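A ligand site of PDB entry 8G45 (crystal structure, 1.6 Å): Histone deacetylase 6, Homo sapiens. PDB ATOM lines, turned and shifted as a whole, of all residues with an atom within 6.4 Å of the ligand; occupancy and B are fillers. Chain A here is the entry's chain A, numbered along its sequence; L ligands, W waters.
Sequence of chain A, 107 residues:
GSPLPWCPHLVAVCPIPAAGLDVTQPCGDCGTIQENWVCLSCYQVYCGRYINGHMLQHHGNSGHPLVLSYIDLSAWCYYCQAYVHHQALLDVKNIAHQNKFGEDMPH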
ATOM      1  N   GLU A  35      22.376 -22.601  26.034  1.00  0.00           N
ATOM      2  CA  GLU A  35      21.171 -21.748  25.873  1.00  0.00           C
ATOM      3  C   GLU A  35      20.467 -21.605  27.219  1.00  0.00           C
ATOM      4  O   GLU A  35      19.251 -21.751  27.264  1.00  0.00           O
ATOM      5  CB  GLU A  35      20.307 -22.328  24.774  1.00  0.00           C
ATOM      6  CG  GLU A  35      21.097 -22.303  23.478  1.00  0.00           C
ATOM      7  CD  GLU A  35      20.271 -22.094  22.221  1.00  0.00           C
ATOM      8  OE1 GLU A  35      19.031 -22.336  22.287  1.00  0.00           O
ATOM      9  OE2 GLU A  35      20.881 -21.716  21.193  1.00  0.00           O
ATOM     10  N   ASN A  36      21.204 -21.181  28.220  1.00  0.00           N
ATOM     11  CA  ASN A  36      20.535 -20.856  29.494  1.00  0.00           C
ATOM     12  C   ASN A  36      19.969 -19.431  29.485  1.00  0.00           C
ATOM     13  O   ASN A  36      20.482 -18.533  28.820  1.00  0.00           O
ATOM     14  CB  ASN A  36      21.447 -21.099  30.682  1.00  0.00           C
ATOM     15  CG  ASN A  36      21.687 -22.578  30.866  1.00  0.00           C
ATOM     16  OD1 ASN A  36      20.741 -23.353  30.951  1.00  0.00           O
ATOM     17  ND2 ASN A  36      22.941 -22.976  30.913  1.00  0.00           N
ATOM     18  N   TRP A  37      18.992 -19.261  30.346  1.00  0.00           N
ATOM     19  CA  TRP A  37      18.311 -18.010  30.648  1.00  0.00           C
ATOM     20  C   TRP A  37      18.381 -17.806  32.145  1.00  0.00           C
ATOM     21  O   TRP A  37      18.425 -18.792  32.879  1.00  0.00           O
ATOM     22  CB  TRP A  37      16.866 -18.037  30.180  1.00  0.00           C
ATOM     23  CG  TRP A  37      16.708 -18.180  28.693  1.00  0.00           C
ATOM     24  CD1 TRP A  37      16.882 -19.328  27.947  1.00  0.00           C
ATOM     25  CD2 TRP A  37      16.289 -17.155  27.791  1.00  0.00           C
ATOM     26  NE1 TRP A  37      16.623 -19.076  26.621  1.00  0.00           N
ATOM     27  CE2 TRP A  37      16.270 -17.745  26.495  1.00  0.00           C
ATOM     28  CE3 TRP A  37      15.948 -15.805  27.939  1.00  0.00           C
ATOM     29  CZ2 TRP A  37      15.853 -17.023  25.379  1.00  0.00           C
ATOM     30  CZ3 TRP A  37      15.550 -15.098  26.822  1.00  0.00           C
ATOM     31  CH2 TRP A  37      15.557 -15.706  25.567  1.00  0.00           C
ATOM     32  N   CYS A  47      17.509 -23.851  31.402  1.00  0.00           N
ATOM     33  CA  CYS A  47      17.800 -23.951  29.950  1.00  0.00           C
ATOM     34  C   CYS A  47      16.559 -23.593  29.135  1.00  0.00           C
ATOM     35  O   CYS A  47      15.394 -23.674  29.558  1.00  0.00           O
ATOM     36  CB  CYS A  47      18.340 -25.351  29.615  1.00  0.00           C
ATOM     37  SG  CYS A  47      17.162 -26.706  29.885  1.00  0.00           S
ATOM     38  N   GLY A  48      16.839 -23.181  27.919  1.00  0.00           N
ATOM     39  CA  GLY A  48      15.825 -22.785  26.961  1.00  0.00           C
ATOM     40  C   GLY A  48      15.057 -23.910  26.340  1.00  0.00           C
ATOM     41  O   GLY A  48      15.421 -25.082  26.496  1.00  0.00           O
ATOM     42  N   ARG A  49      14.021 -23.533  25.588  1.00  0.00           N
ATOM     43  CA  ARG A  49      13.048 -24.484  25.053  1.00  0.00           C
ATOM     44  C   ARG A  49      13.676 -25.431  24.034  1.00  0.00           C
ATOM     45  O   ARG A  49      13.133 -26.566  23.910  1.00  0.00           O
ATOM     46  CB  ARG A  49      11.876 -23.732  24.412  1.00  0.00           C
ATOM     47  CG  ARG A  49      12.269 -22.835  23.272  1.00  0.00           C
ATOM     48  CD  ARG A  49      11.159 -21.840  23.012  1.00  0.00           C
ATOM     49  NE  ARG A  49      11.564 -20.958  21.952  1.00  0.00           N
ATOM     50  CZ  ARG A  49      11.044 -20.958  20.727  1.00  0.00           C
ATOM     51  NH1 ARG A  49      10.140 -21.862  20.386  1.00  0.00           N
ATOM     52  NH2 ARG A  49      11.441 -20.059  19.846  1.00  0.00           N
ATOM     53  N   TYR A  50      14.751 -25.033  23.341  1.00  0.00           N
ATOM     54  CA  TYR A  50      15.411 -25.935  22.359  1.00  0.00           C
ATOM     55  C   TYR A  50      16.335 -26.917  23.047  1.00  0.00           C
ATOM     56  O   TYR A  50      16.786 -27.834  22.345  1.00  0.00           O
ATOM     57  CB  TYR A  50      16.125 -25.131  21.276  1.00  0.00           C
ATOM     58  CG  TYR A  50      15.162 -24.351  20.427  1.00  0.00           C
ATOM     59  CD1 TYR A  50      14.103 -24.986  19.781  1.00  0.00           C
ATOM     60  CD2 TYR A  50      15.288 -22.996  20.261  1.00  0.00           C
ATOM     61  CE1 TYR A  50      13.225 -24.280  18.974  1.00  0.00           C
ATOM     62  CE2 TYR A  50      14.418 -22.275  19.468  1.00  0.00           C
ATOM     63  CZ  TYR A  50      13.371 -22.914  18.826  1.00  0.00           C
ATOM     64  OH  TYR A  50      12.522 -22.185  18.028  1.00  0.00           O
ATOM     65  N   GLY A  53      13.925 -27.192  28.066  1.00  0.00           N
ATOM     66  CA  GLY A  53      12.755 -26.383  28.430  1.00  0.00           C
ATOM     67  C   GLY A  53      12.591 -26.161  29.912  1.00  0.00           C
ATOM     68  O   GLY A  53      11.440 -25.943  30.359  1.00  0.00           O
ATOM     69  N   HIS A  54      13.643 -26.192  30.704  1.00  0.00           N
ATOM     70  CA  HIS A  54      13.519 -26.016  32.165  1.00  0.00           C
ATOM     71  C   HIS A  54      13.115 -24.578  32.551  1.00  0.00           C
ATOM     72  O   HIS A  54      12.480 -24.447  33.605  1.00  0.00           O
ATOM     73  CB  HIS A  54      14.760 -26.495  32.912  1.00  0.00           C
ATOM     74  CG  HIS A  54      14.868 -27.974  32.819  1.00  0.00           C
ATOM     75  ND1 HIS A  54      16.035 -28.610  32.450  1.00  0.00           N
ATOM     76  CD2 HIS A  54      13.916 -28.938  33.019  1.00  0.00           C
ATOM     77  CE1 HIS A  54      15.789 -29.941  32.435  1.00  0.00           C
ATOM     78  NE2 HIS A  54      14.490 -30.154  32.760  1.00  0.00           N
ATOM     79  N   MET A  55      13.485 -23.556  31.749  1.00  0.00           N
ATOM     80  CA  MET A  55      13.071 -22.181  32.104  1.00  0.00           C
ATOM     81  C   MET A  55      11.551 -22.064  31.877  1.00  0.00           C
ATOM     82  O   MET A  55      10.879 -21.437  32.707  1.00  0.00           O
ATOM     83  CB  MET A  55      13.827 -21.060  31.381  1.00  0.00           C
ATOM     84  CG  MET A  55      13.441 -19.656  31.918  1.00  0.00           C
ATOM     85  SD  MET A  55      13.738 -19.471  33.717  1.00  0.00           S
ATOM     86  CE  MET A  55      15.475 -19.087  33.669  1.00  0.00           C
ATOM     87  N   LEU A  56      11.017 -22.646  30.808  1.00  0.00           N
ATOM     88  CA  LEU A  56       9.552 -22.621  30.559  1.00  0.00           C
ATOM     89  C   LEU A  56       8.862 -23.374  31.708  1.00  0.00           C
ATOM     90  O   LEU A  56       7.813 -22.931  32.176  1.00  0.00           O
ATOM     91  CB  LEU A  56       9.246 -23.263  29.197  1.00  0.00           C
ATOM     92  CG  LEU A  56       7.756 -23.445  28.872  1.00  0.00           C
ATOM     93  CD1 LEU A  56       7.018 -22.138  28.978  1.00  0.00           C
ATOM     94  CD2 LEU A  56       7.609 -24.045  27.486  1.00  0.00           C
ATOM     95  N   VAL A  67      12.713 -13.257  31.553  1.00  0.00           N
ATOM     96  CA  VAL A  67      13.968 -14.036  31.631  1.00  0.00           C
ATOM     97  C   VAL A  67      14.920 -13.414  30.615  1.00  0.00           C
ATOM     98  O   VAL A  67      14.509 -12.929  29.581  1.00  0.00           O
ATOM     99  CB  VAL A  67      13.676 -15.536  31.379  1.00  0.00           C
ATOM    100  CG1 VAL A  67      12.786 -16.081  32.490  1.00  0.00           C
ATOM    101  CG2 VAL A  67      13.004 -15.765  29.993  1.00  0.00           C
ATOM    102  N   SER A  69      18.456 -13.877  28.302  1.00  0.00           N
ATOM    103  CA  SER A  69      19.280 -14.854  27.568  1.00  0.00           C
ATOM    104  C   SER A  69      20.758 -14.637  27.855  1.00  0.00           C
ATOM    105  O   SER A  69      21.282 -13.515  27.686  1.00  0.00           O
ATOM    106  CB  SER A  69      19.064 -14.772  26.085  1.00  0.00           C
ATOM    107  OG  SER A  69      20.021 -15.617  25.416  1.00  0.00           O
ATOM    108  N   ILE A  71      22.849 -15.969  25.944  1.00  0.00           N
ATOM    109  CA  ILE A  71      23.430 -15.987  24.556  1.00  0.00           C
ATOM    110  C   ILE A  71      23.517 -14.547  24.073  1.00  0.00           C
ATOM    111  O   ILE A  71      24.624 -14.119  23.674  1.00  0.00           O
ATOM    112  CB  ILE A  71      22.620 -16.860  23.590  1.00  0.00           C
ATOM    113  CG1 ILE A  71      22.528 -18.302  24.086  1.00  0.00           C
ATOM    114  CG2 ILE A  71      23.169 -16.793  22.155  1.00  0.00           C
ATOM    115  CD1 ILE A  71      23.818 -18.861  24.616  1.00  0.00           C
ATOM    116  N   ASP A  72      22.406 -13.818  24.012  1.00  0.00           N
ATOM    117  CA  ASP A  72      22.458 -12.466  23.373  1.00  0.00           C
ATOM    118  C   ASP A  72      21.891 -11.358  24.258  1.00  0.00           C
ATOM    119  O   ASP A  72      21.735 -10.231  23.733  1.00  0.00           O
ATOM    120  CB  ASP A  72      21.720 -12.511  22.035  1.00  0.00           C
ATOM    121  CG  ASP A  72      20.213 -12.492  22.197  1.00  0.00           C
ATOM    122  OD1 ASP A  72      19.712 -12.885  23.303  1.00  0.00           O
ATOM    123  OD2 ASP A  72      19.546 -12.036  21.263  1.00  0.00           O
ATOM    124  N   LEU A  73      21.627 -11.623  25.545  1.00  0.00           N
ATOM    125  CA  LEU A  73      21.193 -10.608  26.537  1.00  0.00           C
ATOM    126  C   LEU A  73      19.846 -10.013  26.121  1.00  0.00           C
ATOM    127  O   LEU A  73      19.573  -8.880  26.539  1.00  0.00           O
ATOM    128  CB  LEU A  73      22.245  -9.517  26.684  1.00  0.00           C
ATOM    129  CG  LEU A  73      23.664 -10.037  26.917  1.00  0.00           C
ATOM    130  CD1 LEU A  73      24.595  -8.886  27.224  1.00  0.00           C
ATOM    131  CD2 LEU A  73      23.718 -11.067  28.040  1.00  0.00           C
ATOM    132  N   SER A  74      19.032 -10.734  25.382  1.00  0.00           N
ATOM    133  CA  SER A  74      17.650 -10.300  25.080  1.00  0.00           C
ATOM    134  C   SER A  74      16.766 -10.736  26.251  1.00  0.00           C
ATOM    135  O   SER A  74      17.086 -11.742  26.893  1.00  0.00           O
ATOM    136  CB  SER A  74      17.183 -10.817  23.793  1.00  0.00           C
ATOM    137  OG  SER A  74      17.023 -12.205  23.916  1.00  0.00           O
ATOM    138  N   TRP A  76      12.928 -11.897  27.489  1.00  0.00           N
ATOM    139  CA  TRP A  76      11.684 -12.507  26.992  1.00  0.00           C
ATOM    140  C   TRP A  76      10.647 -12.442  28.098  1.00  0.00           C
ATOM    141  O   TRP A  76      10.956 -12.817  29.246  1.00  0.00           O
ATOM    142  CB  TRP A  76      11.921 -13.955  26.553  1.00  0.00           C
ATOM    143  CG  TRP A  76      10.714 -14.642  26.035  1.00  0.00           C
ATOM    144  CD1 TRP A  76       9.946 -15.521  26.739  1.00  0.00           C
ATOM    145  CD2 TRP A  76      10.099 -14.497  24.752  1.00  0.00           C
ATOM    146  NE1 TRP A  76       8.881 -15.923  25.986  1.00  0.00           N
ATOM    147  CE2 TRP A  76       8.980 -15.353  24.739  1.00  0.00           C
ATOM    148  CE3 TRP A  76      10.401 -13.767  23.598  1.00  0.00           C
ATOM    149  CZ2 TRP A  76       8.144 -15.491  23.632  1.00  0.00           C
ATOM    150  CZ3 TRP A  76       9.568 -13.908  22.499  1.00  0.00           C
ATOM    151  CH2 TRP A  76       8.479 -14.749  22.525  1.00  0.00           C
ATOM    152  N   TYR A  78       7.211 -14.227  29.123  1.00  0.00           N
ATOM    153  CA  TYR A  78       6.404 -15.438  28.814  1.00  0.00           C
ATOM    154  C   TYR A  78       4.907 -15.098  28.682  1.00  0.00           C
ATOM    155  O   TYR A  78       4.196 -15.779  27.940  1.00  0.00           O
ATOM    156  CB  TYR A  78       6.558 -16.519  29.879  1.00  0.00           C
ATOM    157  CG  TYR A  78       7.848 -17.276  29.804  1.00  0.00           C
ATOM    158  CD1 TYR A  78       8.063 -18.224  28.797  1.00  0.00           C
ATOM    159  CD2 TYR A  78       8.840 -17.082  30.724  1.00  0.00           C
ATOM    160  CE1 TYR A  78       9.259 -18.935  28.719  1.00  0.00           C
ATOM    161  CE2 TYR A  78      10.018 -17.770  30.650  1.00  0.00           C
ATOM    162  CZ  TYR A  78      10.213 -18.721  29.672  1.00  0.00           C
ATOM    163  OH  TYR A  78      11.382 -19.399  29.651  1.00  0.00           O
ATOM    164  N   GLN A  81       4.609 -12.921  25.432  1.00  0.00           N
ATOM    165  CA  GLN A  81       5.154 -13.736  24.312  1.00  0.00           C
ATOM    166  C   GLN A  81       5.900 -12.780  23.384  1.00  0.00           C
ATOM    167  O   GLN A  81       5.687 -12.807  22.143  1.00  0.00           O
ATOM    168  CB  GLN A  81       4.091 -14.579  23.613  1.00  0.00           C
ATOM    169  CG  GLN A  81       3.160 -15.272  24.595  1.00  0.00           C
ATOM    170  CD  GLN A  81       1.936 -15.829  23.927  1.00  0.00           C
ATOM    171  OE1 GLN A  81       0.824 -15.297  24.044  1.00  0.00           O
ATOM    172  NE2 GLN A  81       2.130 -16.895  23.180  1.00  0.00           N
ATOM    173  N   TYR A  83       9.811 -10.164  23.146  1.00  0.00           N
ATOM    174  CA  TYR A  83      11.001  -9.548  23.747  1.00  0.00           C
ATOM    175  C   TYR A  83      10.607  -8.164  24.245  1.00  0.00           C
ATOM    176  O   TYR A  83       9.726  -7.527  23.653  1.00  0.00           O
ATOM    177  CB  TYR A  83      12.116  -9.414  22.739  1.00  0.00           C
ATOM    178  CG  TYR A  83      12.584 -10.746  22.219  1.00  0.00           C
ATOM    179  CD1 TYR A  83      13.499 -11.481  22.943  1.00  0.00           C
ATOM    180  CD2 TYR A  83      12.166 -11.225  20.983  1.00  0.00           C
ATOM    181  CE1 TYR A  83      14.003 -12.667  22.440  1.00  0.00           C
ATOM    182  CE2 TYR A  83      12.603 -12.447  20.515  1.00  0.00           C
ATOM    183  CZ  TYR A  83      13.544 -13.156  21.239  1.00  0.00           C
ATOM    184  OH  TYR A  83      14.009 -14.346  20.749  1.00  0.00           O
HETATM  185  C1  LIG L   1      17.425 -16.998  21.786  1.00  0.00           C
HETATM  186  C2  LIG L   1      18.516 -17.348  22.582  1.00  0.00           C
HETATM  187  C3  LIG L   1      18.741 -18.669  22.864  1.00  0.00           C
HETATM  188  C4  LIG L   1      17.898 -19.645  22.382  1.00  0.00           C
HETATM  189  C5  LIG L   1      16.825 -19.310  21.584  1.00  0.00           C
HETATM  190  C6  LIG L   1      16.585 -17.985  21.265  1.00  0.00           C
HETATM  191  C7  LIG L   1      15.386 -17.586  20.460  1.00  0.00           C
HETATM  192  N1  LIG L   1      11.482 -17.450  23.206  1.00  0.00           N
HETATM  193  N2  LIG L   1      10.390 -18.857  24.727  1.00  0.00           N
HETATM  194  C8  LIG L   1      13.565 -17.579  22.077  1.00  0.00           C
HETATM  195  C9  LIG L   1      12.640 -16.681  22.878  1.00  0.00           C
HETATM  196  C10 LIG L   1      11.370 -18.093  24.420  1.00  0.00           C
HETATM  197  C11 LIG L   1      12.544 -17.932  25.337  1.00  0.00           C
HETATM  198  C12 LIG L   1      12.401 -18.686  26.636  1.00  0.00           C
HETATM  199  C13 LIG L   1      12.585 -20.208  26.554  1.00  0.00           C
HETATM  200  C14 LIG L   1       9.350 -18.985  23.804  1.00  0.00           C
HETATM  201  O1  LIG L   1      13.477 -18.821  22.146  1.00  0.00           O
HETATM  202  N3  LIG L   1      14.427 -16.921  21.325  1.00  0.00           N
HETATM  203  O2  LIG L   1      17.021 -15.723  21.558  1.00  0.00           O
HETATM  204  C15 LIG L   1      17.732 -14.678  22.172  1.00  0.00           C
HETATM  205  C16 LIG L   1      10.510 -17.575  22.213  1.00  0.00           C
HETATM  206  O3  LIG L   1      10.729 -17.173  21.085  1.00  0.00           O
HETATM  207  C17 LIG L   1       9.374 -18.346  22.566  1.00  0.00           C
HETATM  208  C18 LIG L   1       8.333 -18.496  21.647  1.00  0.00           C
HETATM  209  C19 LIG L   1       7.281 -19.340  21.963  1.00  0.00           C
HETATM  210  C20 LIG L   1       7.247 -20.008  23.161  1.00  0.00           C
HETATM  211  C21 LIG L   1       8.267 -19.818  24.069  1.00  0.00           C
HETATM  212 CL1  LIG L   1       8.166 -20.564  25.615  1.00  0.00          CL
HETATM  213  O4  LIG L   1      13.271 -20.752  25.681  1.00  0.00           O
HETATM  214  O5  LIG L   1      12.032 -20.825  27.552  1.00  0.00           O
HETATM  215  O   HOH W   1      15.256 -20.400  24.165  1.00  0.00           O
HETATM  216  O   HOH W   2      12.687 -23.227  28.575  1.00  0.00           O
HETATM  217  O   HOH W   3      19.726 -18.290  26.120  1.00  0.00           O
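OH of Tyr 83 sits at hydrogen-bond distance from N3 of the ligand (2.7 Å). The backbone NH (N) of Arg 49 lies within hydrogen-bond range of an oxygen (O4) of the ligand (2.9 Å). An oxygen (O5) of the ligand is in hydrogen-bond range of the side-chain hydroxyl (OH) of Tyr 78 (2.6 Å). The guanidinium group of Arg 49 lies within hydrogen-bond range of an oxygen (O1) of the ligand.
OE1 of Glu 35 touches C4 of the ligand, at 2.9 Å. Trp 37 touches the ligand. Gly 48 touches the ligand. Leu 56 touches the ligand. Ser 69 touches the ligand. Ile 71 touches the ligand (CG1 to C3, 3.996 Å). Asp 72 touches the ligand. OG of Ser 74 touches C15 of the ligand, 3.1 Å away. CZ2 of Trp 76 touches C17 of the ligand (3.3 Å). Within 4 Å of the ligand: Glu 35, Trp 37, Gly 48, Arg 49, Leu 56, Ser 69, Ile 71, Asp 72, Ser 74, Trp 76, Tyr 78 and Tyr 83.
Water W1 bridges an oxygen (O4) of the ligand and the indole nitrogen of Trp 37. Water W3 lies within hydrogen-bond range of the side-chain hydroxyl of Ser 69 (2.8 Å), the backbone carbonyl oxygen of Asn 36 (2.8 Å) and the indole nitrogen of Trp 37 (3.2 Å).
The side-chain hydroxyl (OG) of Ser 74 is in hydrogen-bond range of the side-chain carboxylate (OD1) of Asp 72 (2.8 Å). OG of Ser 69 is in hydrogen-bond range of N of Ile 71 (2.9 Å). The backbone carbonyl oxygen of Gly 48 sits at hydrogen-bond distance from the backbone NH of Gly 53, at 3.0 Å. N of Gly 48 sits at hydrogen-bond distance from O of Glu 35 (2.9 Å). N of Leu 56 is in hydrogen-bond range of OH of Tyr 78, at 3.5 Å. The guanidinium group (NH2) of Arg 49 is in hydrogen-bond range of the side-chain hydroxyl (OH) of Tyr 50 (3.0 Å). N of Trp 76 is in hydrogen-bond range of O of Val 67. N of Asp 72 sits at hydrogen-bond distance from OG of Ser 69.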
